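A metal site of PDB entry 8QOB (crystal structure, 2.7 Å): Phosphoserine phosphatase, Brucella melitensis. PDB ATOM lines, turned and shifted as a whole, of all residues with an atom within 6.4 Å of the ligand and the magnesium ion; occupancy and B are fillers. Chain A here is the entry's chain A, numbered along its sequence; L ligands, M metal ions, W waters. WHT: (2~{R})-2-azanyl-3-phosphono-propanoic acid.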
ATOM      1  N   ASP A  98      17.795  29.226   0.498  1.00  0.00           N
ATOM      2  CA  ASP A  98      18.780  29.108   1.561  1.00  0.00           C
ATOM      3  C   ASP A  98      19.777  30.279   1.526  1.00  0.00           C
ATOM      4  O   ASP A  98      20.079  30.833   0.475  1.00  0.00           O
ATOM      5  CB  ASP A  98      19.524  27.804   1.365  1.00  0.00           C
ATOM      6  CG  ASP A  98      20.382  27.486   2.520  1.00  0.00           C
ATOM      7  OD1 ASP A  98      19.888  27.642   3.665  1.00  0.00           O
ATOM      8  OD2 ASP A  98      21.562  27.127   2.276  1.00  0.00           O
ATOM      9  N   MET A  99      20.294  30.649   2.699  1.00  0.00           N
ATOM     10  CA  MET A  99      21.379  31.640   2.699  1.00  0.00           C
ATOM     11  C   MET A  99      22.773  31.015   2.660  1.00  0.00           C
ATOM     12  O   MET A  99      23.419  31.034   1.608  1.00  0.00           O
ATOM     13  CB  MET A  99      21.271  32.586   3.886  1.00  0.00           C
ATOM     14  CG  MET A  99      22.043  33.884   3.646  1.00  0.00           C
ATOM     15  SD  MET A  99      22.534  34.819   5.125  1.00  0.00           S
ATOM     16  CE  MET A  99      23.170  33.522   6.201  1.00  0.00           C
ATOM     17  N   ASP A 100      23.233  30.493   3.798  1.00  0.00           N
ATOM     18  CA  ASP A 100      24.602  29.981   3.925  1.00  0.00           C
ATOM     19  C   ASP A 100      24.943  29.009   2.803  1.00  0.00           C
ATOM     20  O   ASP A 100      24.215  28.041   2.570  1.00  0.00           O
ATOM     21  CB  ASP A 100      24.776  29.275   5.269  1.00  0.00           C
ATOM     22  CG  ASP A 100      25.140  30.206   6.387  1.00  0.00           C
ATOM     23  OD1 ASP A 100      25.309  31.414   6.126  1.00  0.00           O
ATOM     24  OD2 ASP A 100      25.270  29.736   7.527  1.00  0.00           O
ATOM     25  N   SER A 101      26.060  29.273   2.130  1.00  0.00           N
ATOM     26  CA  SER A 101      26.618  28.466   1.035  1.00  0.00           C
ATOM     27  C   SER A 101      25.770  28.442  -0.228  1.00  0.00           C
ATOM     28  O   SER A 101      26.214  27.915  -1.248  1.00  0.00           O
ATOM     29  CB  SER A 101      26.864  27.012   1.491  1.00  0.00           C
ATOM     30  OG  SER A 101      28.097  26.911   2.170  1.00  0.00           O
ATOM     31  N   THR A 102      24.556  28.985  -0.200  1.00  0.00           N
ATOM     32  CA  THR A 102      23.750  29.104  -1.413  1.00  0.00           C
ATOM     33  C   THR A 102      23.811  30.507  -1.992  1.00  0.00           C
ATOM     34  O   THR A 102      24.214  30.688  -3.147  1.00  0.00           O
ATOM     35  CB  THR A 102      22.291  28.680  -1.146  1.00  0.00           C
ATOM     36  OG1 THR A 102      22.242  27.275  -0.853  1.00  0.00           O
ATOM     37  CG2 THR A 102      21.439  28.952  -2.364  1.00  0.00           C
ATOM     38  N   GLU A 107      29.758  29.843   5.385  1.00  0.00           N
ATOM     39  CA  GLU A 107      28.880  29.428   6.468  1.00  0.00           C
ATOM     40  C   GLU A 107      29.044  30.451   7.585  1.00  0.00           C
ATOM     41  O   GLU A 107      30.130  30.558   8.180  1.00  0.00           O
ATOM     42  CB  GLU A 107      29.241  28.020   6.965  1.00  0.00           C
ATOM     43  CG  GLU A 107      29.155  26.947   5.882  1.00  0.00           C
ATOM     44  CD  GLU A 107      27.730  26.520   5.586  1.00  0.00           C
ATOM     45  OE1 GLU A 107      26.807  26.880   6.368  1.00  0.00           O
ATOM     46  OE2 GLU A 107      27.529  25.823   4.573  1.00  0.00           O
ATOM     47  N   CYS A 108      27.969  31.222   7.853  1.00  0.00           N
ATOM     48  CA  CYS A 108      28.015  32.282   8.866  1.00  0.00           C
ATOM     49  C   CYS A 108      28.433  31.719  10.232  1.00  0.00           C
ATOM     50  O   CYS A 108      29.184  32.367  10.962  1.00  0.00           O
ATOM     51  CB  CYS A 108      26.667  33.043   8.932  1.00  0.00           C
ATOM     52  SG  CYS A 108      25.034  32.265   9.511  1.00  0.00           S
ATOM     53  N   ILE A 109      27.994  30.506  10.545  1.00  0.00           N
ATOM     54  CA  ILE A 109      28.371  29.836  11.794  1.00  0.00           C
ATOM     55  C   ILE A 109      29.880  29.558  11.827  1.00  0.00           C
ATOM     56  O   ILE A 109      30.545  29.808  12.847  1.00  0.00           O
ATOM     57  CB  ILE A 109      27.515  28.563  11.976  1.00  0.00           C
ATOM     58  CG1 ILE A 109      27.866  27.820  13.267  1.00  0.00           C
ATOM     59  CG2 ILE A 109      27.619  27.660  10.745  1.00  0.00           C
ATOM     60  CD1 ILE A 109      27.610  28.595  14.509  1.00  0.00           C
ATOM     61  N   ASP A 110      30.449  29.061  10.724  1.00  0.00           N
ATOM     62  CA  ASP A 110      31.872  28.703  10.671  1.00  0.00           C
ATOM     63  C   ASP A 110      32.780  29.941  10.756  1.00  0.00           C
ATOM     64  O   ASP A 110      33.921  29.848  11.233  1.00  0.00           O
ATOM     65  CB  ASP A 110      32.188  27.936   9.366  1.00  0.00           C
ATOM     66  CG  ASP A 110      31.603  26.512   9.342  1.00  0.00           C
ATOM     67  OD1 ASP A 110      30.925  26.110  10.324  1.00  0.00           O
ATOM     68  OD2 ASP A 110      31.828  25.780   8.346  1.00  0.00           O
ATOM     69  N   THR A 126      29.476  21.454  11.018  1.00  0.00           N
ATOM     70  CA  THR A 126      28.661  22.019   9.940  1.00  0.00           C
ATOM     71  C   THR A 126      28.579  21.063   8.752  1.00  0.00           C
ATOM     72  O   THR A 126      27.493  20.762   8.259  1.00  0.00           O
ATOM     73  CB  THR A 126      29.238  23.361   9.506  1.00  0.00           C
ATOM     74  OG1 THR A 126      29.116  24.289  10.593  1.00  0.00           O
ATOM     75  CG2 THR A 126      28.484  23.909   8.298  1.00  0.00           C
ATOM     76  N   ALA A 129      26.305  18.187   9.633  1.00  0.00           N
ATOM     77  CA  ALA A 129      24.924  18.665   9.669  1.00  0.00           C
ATOM     78  C   ALA A 129      24.369  18.813   8.260  1.00  0.00           C
ATOM     79  O   ALA A 129      23.303  18.291   7.937  1.00  0.00           O
ATOM     80  CB  ALA A 129      24.847  19.997  10.417  1.00  0.00           C
ATOM     81  N   MET A 130      25.106  19.527   7.400  1.00  0.00           N
ATOM     82  CA  MET A 130      24.608  19.814   6.075  1.00  0.00           C
ATOM     83  C   MET A 130      24.598  18.586   5.160  1.00  0.00           C
ATOM     84  O   MET A 130      23.932  18.623   4.114  1.00  0.00           O
ATOM     85  CB  MET A 130      25.413  20.957   5.462  1.00  0.00           C
ATOM     86  CG  MET A 130      25.293  22.222   6.324  1.00  0.00           C
ATOM     87  SD  MET A 130      23.619  22.949   6.188  1.00  0.00           S
ATOM     88  CE  MET A 130      23.050  22.559   7.840  1.00  0.00           C
ATOM     89  N   PHE A 136      19.652  19.078  12.471  1.00  0.00           N
ATOM     90  CA  PHE A 136      20.132  20.455  12.435  1.00  0.00           C
ATOM     91  C   PHE A 136      20.172  21.070  13.820  1.00  0.00           C
ATOM     92  O   PHE A 136      21.113  21.807  14.144  1.00  0.00           O
ATOM     93  CB  PHE A 136      19.264  21.312  11.524  1.00  0.00           C
ATOM     94  CG  PHE A 136      19.755  22.717  11.422  1.00  0.00           C
ATOM     95  CD1 PHE A 136      20.885  23.018  10.662  1.00  0.00           C
ATOM     96  CD2 PHE A 136      19.118  23.733  12.126  1.00  0.00           C
ATOM     97  CE1 PHE A 136      21.361  24.320  10.583  1.00  0.00           C
ATOM     98  CE2 PHE A 136      19.581  25.051  12.040  1.00  0.00           C
ATOM     99  CZ  PHE A 136      20.697  25.349  11.282  1.00  0.00           C
ATOM    100  N   LEU A 140      23.173  22.986  15.588  1.00  0.00           N
ATOM    101  CA  LEU A 140      23.198  24.408  15.894  1.00  0.00           C
ATOM    102  C   LEU A 140      23.558  24.637  17.348  1.00  0.00           C
ATOM    103  O   LEU A 140      24.464  25.417  17.657  1.00  0.00           O
ATOM    104  CB  LEU A 140      21.854  25.054  15.566  1.00  0.00           C
ATOM    105  CG  LEU A 140      21.937  26.558  15.385  1.00  0.00           C
ATOM    106  CD1 LEU A 140      23.104  26.897  14.441  1.00  0.00           C
ATOM    107  CD2 LEU A 140      20.633  27.112  14.831  1.00  0.00           C
ATOM    108  N   ARG A 143      27.296  23.935  18.021  1.00  0.00           N
ATOM    109  CA  ARG A 143      28.196  24.914  17.426  1.00  0.00           C
ATOM    110  C   ARG A 143      28.038  26.291  18.075  1.00  0.00           C
ATOM    111  O   ARG A 143      29.028  26.937  18.422  1.00  0.00           O
ATOM    112  CB  ARG A 143      27.958  24.991  15.914  1.00  0.00           C
ATOM    113  CG  ARG A 143      28.465  23.773  15.124  1.00  0.00           C
ATOM    114  CD  ARG A 143      27.972  23.851  13.678  1.00  0.00           C
ATOM    115  NE  ARG A 143      26.524  23.679  13.586  1.00  0.00           N
ATOM    116  CZ  ARG A 143      25.816  23.880  12.486  1.00  0.00           C
ATOM    117  NH1 ARG A 143      26.374  24.346  11.384  1.00  0.00           N
ATOM    118  NH2 ARG A 143      24.515  23.600  12.488  1.00  0.00           N
ATOM    119  N   VAL A 186      15.356  32.186   3.470  1.00  0.00           N
ATOM    120  CA  VAL A 186      14.974  31.348   4.599  1.00  0.00           C
ATOM    121  C   VAL A 186      16.165  30.465   4.994  1.00  0.00           C
ATOM    122  O   VAL A 186      16.521  29.528   4.268  1.00  0.00           O
ATOM    123  CB  VAL A 186      13.725  30.507   4.274  1.00  0.00           C
ATOM    124  CG1 VAL A 186      13.276  29.726   5.473  1.00  0.00           C
ATOM    125  CG2 VAL A 186      12.627  31.446   3.777  1.00  0.00           C
ATOM    126  N   SER A 187      16.732  30.755   6.169  1.00  0.00           N
ATOM    127  CA  SER A 187      18.030  30.259   6.607  1.00  0.00           C
ATOM    128  C   SER A 187      17.905  29.628   7.992  1.00  0.00           C
ATOM    129  O   SER A 187      17.031  29.988   8.796  1.00  0.00           O
ATOM    130  CB  SER A 187      19.052  31.446   6.607  1.00  0.00           C
ATOM    131  OG  SER A 187      20.261  31.182   7.298  1.00  0.00           O
ATOM    132  N   GLY A 188      18.766  28.631   8.255  1.00  0.00           N
ATOM    133  CA  GLY A 188      19.006  28.139   9.591  1.00  0.00           C
ATOM    134  C   GLY A 188      20.060  28.919  10.335  1.00  0.00           C
ATOM    135  O   GLY A 188      20.460  28.563  11.444  1.00  0.00           O
ATOM    136  N   GLY A 189      20.525  30.003   9.723  1.00  0.00           N
ATOM    137  CA  GLY A 189      21.543  30.837  10.302  1.00  0.00           C
ATOM    138  C   GLY A 189      20.927  31.912  11.158  1.00  0.00           C
ATOM    139  O   GLY A 189      19.945  31.654  11.853  1.00  0.00           O
ATOM    140  N   PHE A 190      21.463  33.126  11.128  1.00  0.00           N
ATOM    141  CA  PHE A 190      21.143  34.075  12.174  1.00  0.00           C
ATOM    142  C   PHE A 190      20.606  35.375  11.587  1.00  0.00           C
ATOM    143  O   PHE A 190      21.110  35.861  10.573  1.00  0.00           O
ATOM    144  CB  PHE A 190      22.372  34.296  13.042  1.00  0.00           C
ATOM    145  CG  PHE A 190      22.975  32.997  13.513  1.00  0.00           C
ATOM    146  CD1 PHE A 190      22.265  32.159  14.356  1.00  0.00           C
ATOM    147  CD2 PHE A 190      24.223  32.586  13.056  1.00  0.00           C
ATOM    148  CE1 PHE A 190      22.788  30.947  14.786  1.00  0.00           C
ATOM    149  CE2 PHE A 190      24.763  31.360  13.480  1.00  0.00           C
ATOM    150  CZ  PHE A 190      24.049  30.549  14.337  1.00  0.00           C
ATOM    151  N   THR A 194      21.020  37.424   7.996  1.00  0.00           N
ATOM    152  CA  THR A 194      20.035  37.372   6.912  1.00  0.00           C
ATOM    153  C   THR A 194      19.369  38.721   6.679  1.00  0.00           C
ATOM    154  O   THR A 194      19.014  39.040   5.529  1.00  0.00           O
ATOM    155  CB  THR A 194      18.977  36.303   7.221  1.00  0.00           C
ATOM    156  OG1 THR A 194      18.382  36.556   8.504  1.00  0.00           O
ATOM    157  CG2 THR A 194      19.602  34.900   7.168  1.00  0.00           C
ATOM    158  N   LYS A 232      11.691  25.259   7.486  1.00  0.00           N
ATOM    159  CA  LYS A 232      11.781  25.777   6.122  1.00  0.00           C
ATOM    160  C   LYS A 232      10.572  25.349   5.290  1.00  0.00           C
ATOM    161  O   LYS A 232      10.089  26.113   4.460  1.00  0.00           O
ATOM    162  CB  LYS A 232      13.104  25.350   5.455  1.00  0.00           C
ATOM    163  CG  LYS A 232      14.338  26.050   6.029  1.00  0.00           C
ATOM    164  CD  LYS A 232      15.506  26.159   5.034  1.00  0.00           C
ATOM    165  CE  LYS A 232      16.864  26.233   5.774  1.00  0.00           C
ATOM    166  NZ  LYS A 232      17.852  27.178   5.167  1.00  0.00           N
ATOM    167  N   GLY A 254      18.682  25.218  -2.359  1.00  0.00           N
ATOM    168  CA  GLY A 254      19.614  25.149  -1.239  1.00  0.00           C
ATOM    169  C   GLY A 254      20.644  24.065  -1.518  1.00  0.00           C
ATOM    170  O   GLY A 254      20.647  23.438  -2.580  1.00  0.00           O
ATOM    171  N   ASP A 255      21.509  23.844  -0.519  1.00  0.00           N
ATOM    172  CA  ASP A 255      22.668  22.965  -0.636  1.00  0.00           C
ATOM    173  C   ASP A 255      22.730  21.855   0.416  1.00  0.00           C
ATOM    174  O   ASP A 255      23.451  20.876   0.197  1.00  0.00           O
ATOM    175  CB  ASP A 255      23.955  23.794  -0.516  1.00  0.00           C
ATOM    176  CG  ASP A 255      24.206  24.310   0.916  1.00  0.00           C
ATOM    177  OD1 ASP A 255      23.341  25.035   1.460  1.00  0.00           O
ATOM    178  OD2 ASP A 255      25.269  23.988   1.508  1.00  0.00           O
ATOM    179  N   GLY A 256      22.039  21.996   1.557  1.00  0.00           N
ATOM    180  CA  GLY A 256      22.229  21.105   2.667  1.00  0.00           C
ATOM    181  C   GLY A 256      20.910  20.407   3.014  1.00  0.00           C
ATOM    182  O   GLY A 256      19.854  20.739   2.472  1.00  0.00           O
ATOM    183  N   ASN A 258      18.963  20.536   5.476  1.00  0.00           N
ATOM    184  CA  ASN A 258      17.871  21.336   6.044  1.00  0.00           C
ATOM    185  C   ASN A 258      17.031  22.004   4.962  1.00  0.00           C
ATOM    186  O   ASN A 258      16.011  22.624   5.292  1.00  0.00           O
ATOM    187  CB  ASN A 258      18.408  22.411   7.008  1.00  0.00           C
ATOM    188  CG  ASN A 258      19.589  23.181   6.454  1.00  0.00           C
ATOM    189  OD1 ASN A 258      20.384  22.644   5.671  1.00  0.00           O
ATOM    190  ND2 ASN A 258      19.699  24.451   6.825  1.00  0.00           N
ATOM    191  N   ASP A 259      17.445  21.942   3.710  1.00  0.00           N
ATOM    192  CA  ASP A 259      16.659  22.453   2.597  1.00  0.00           C
ATOM    193  C   ASP A 259      15.873  21.355   1.892  1.00  0.00           C
ATOM    194  O   ASP A 259      15.085  21.675   0.989  1.00  0.00           O
ATOM    195  CB  ASP A 259      17.557  23.181   1.593  1.00  0.00           C
ATOM    196  CG  ASP A 259      18.353  24.306   2.231  1.00  0.00           C
ATOM    197  OD1 ASP A 259      17.715  25.216   2.802  1.00  0.00           O
ATOM    198  OD2 ASP A 259      19.604  24.283   2.128  1.00  0.00           O
ATOM    199  N   LYS A 275      25.683  19.057  -1.117  1.00  0.00           N
ATOM    200  CA  LYS A 275      26.487  18.075  -0.433  1.00  0.00           C
ATOM    201  C   LYS A 275      26.210  16.670  -0.997  1.00  0.00           C
ATOM    202  O   LYS A 275      25.154  16.423  -1.612  1.00  0.00           O
ATOM    203  CB  LYS A 275      26.200  18.155   1.077  1.00  0.00           C
ATOM    204  CG  LYS A 275      27.080  19.162   1.857  1.00  0.00           C
ATOM    205  CD  LYS A 275      26.789  20.583   1.431  1.00  0.00           C
ATOM    206  CE  LYS A 275      27.620  21.620   2.188  1.00  0.00           C
ATOM    207  NZ  LYS A 275      27.939  22.764   1.270  1.00  0.00           N
HETATM  208  C01 WHT L   1      22.510  27.713   7.828  1.00  0.00           C
HETATM  209  C02 WHT L   1      23.822  26.855   7.917  1.00  0.00           C
HETATM  210  C03 WHT L   1      24.167  26.108   9.251  1.00  0.00           C
HETATM  211  N06 WHT L   1      23.970  25.941   6.788  1.00  0.00           N
HETATM  212  O04 WHT L   1      24.854  25.028   9.270  1.00  0.00           O
HETATM  213  O05 WHT L   1      23.813  26.560  10.379  1.00  0.00           O
HETATM  214  O08 WHT L   1      22.269  27.237   5.051  1.00  0.00           O
HETATM  215  O09 WHT L   1      20.204  27.124   6.384  1.00  0.00           O
HETATM  216  O10 WHT L   1      21.237  29.293   5.702  1.00  0.00           O
HETATM  217  P07 WHT L   1      21.524  27.881   6.198  1.00  0.00           P
HETATM  218 MG    MG M   1      23.177  26.203   3.213  1.00  0.00          MG
HETATM  219  O   HOH W   1      24.902  25.080   3.774  1.00  0.00           O
HETATM  220  O   HOH W   2      21.373  24.624   3.661  1.00  0.00           O
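The backbone NH of Asp 100 sits at hydrogen-bond distance from an oxygen (O10) of the ligand, 3.0 Å away.
The side-chain amino group of Lys 232 lies within salt-bridge range of an oxygen (O09) of the ligand (2.6 Å).
An oxygen (O10) of the ligand lies within hydrogen-bond range of the side-chain hydroxyl (OG) of Ser 187 (2.7 Å).
An oxygen (O04) of the ligand lies within salt-bridge range of the guanidinium group (NH1) of Arg 143, 2.7 Å away.
The side-chain amide nitrogen (ND2) of Asn 258 is in hydrogen-bond range of an oxygen (O09) of the ligand, 2.8 Å away.
O09 of the ligand is in hydrogen-bond range of N of Gly 188, 2.8 Å away.
The side-chain carboxylate (OE1) of Glu 107 is in salt-bridge range of a nitrogen (N06) of the ligand (3.0 Å).
The side-chain sulfur (SD) of Met 130 is in hydrogen-bond range of a nitrogen (N06) of the ligand (3.1 Å).
The backbone NH (N) of Met 99 sits at hydrogen-bond distance from an oxygen (O10) of the ligand (3.4 Å).
Residues that only touch the ligand: Ile 109 (3.98 Å), Thr 126 (3.9 Å), Phe 136 (3.3 Å) and Gly 189 (3.6 Å).
The nearest printed residue that does not touch the ligand is Leu 140 (4.1 Å).
The side-chain amino group (NZ) of Lys 232 is in salt-bridge range of the side-chain carboxylate (OD1) of Asp 98, 2.6 Å away.
The side-chain carboxylate (OD2) of Asp 255 lies within salt-bridge range of the side-chain amino group (NZ) of Lys 275 (2.9 Å).
The side-chain carboxylate of Asp 100 sits at hydrogen-bond distance from the backbone NH of Cys 108 (3.1 Å).
NZ of Lys 232 sits at hydrogen-bond distance from O of Val 186 (2.8 Å).
N of Gly 189 sits at hydrogen-bond distance from OG of Ser 187, 2.7 Å away.
OG1 of Thr 126 sits at hydrogen-bond distance from NH1 of Arg 143.
OE2 of Glu 107 lies within hydrogen-bond range of OG of Ser 101, at 2.7 Å.
The side-chain carboxylate (OD1) of Asp 110 is in hydrogen-bond range of the side-chain hydroxyl (OG1) of Thr 126 (2.6 Å).
OD2 of Asp 98 is bound to the magnesium ion.
The magnesium ion is bound by OD1 of Asp 255, 2.1 Å away.
Water W1 binds the magnesium ion, 2.1 Å away.
O of Asp 100 binds the magnesium ion.
An oxygen (O08) of the ligand is bound to the magnesium ion.
Water W2 binds the magnesium ion, 2.4 Å away.
The magnesium ion has six donor atoms within binding distance.
Three residues have an atom within 4 Å of the magnesium ion: Asp 98, Asp 100 and Asp 255.
The nearest printed residue that does not touch the magnesium ion is Ser 101 (4.1 Å).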
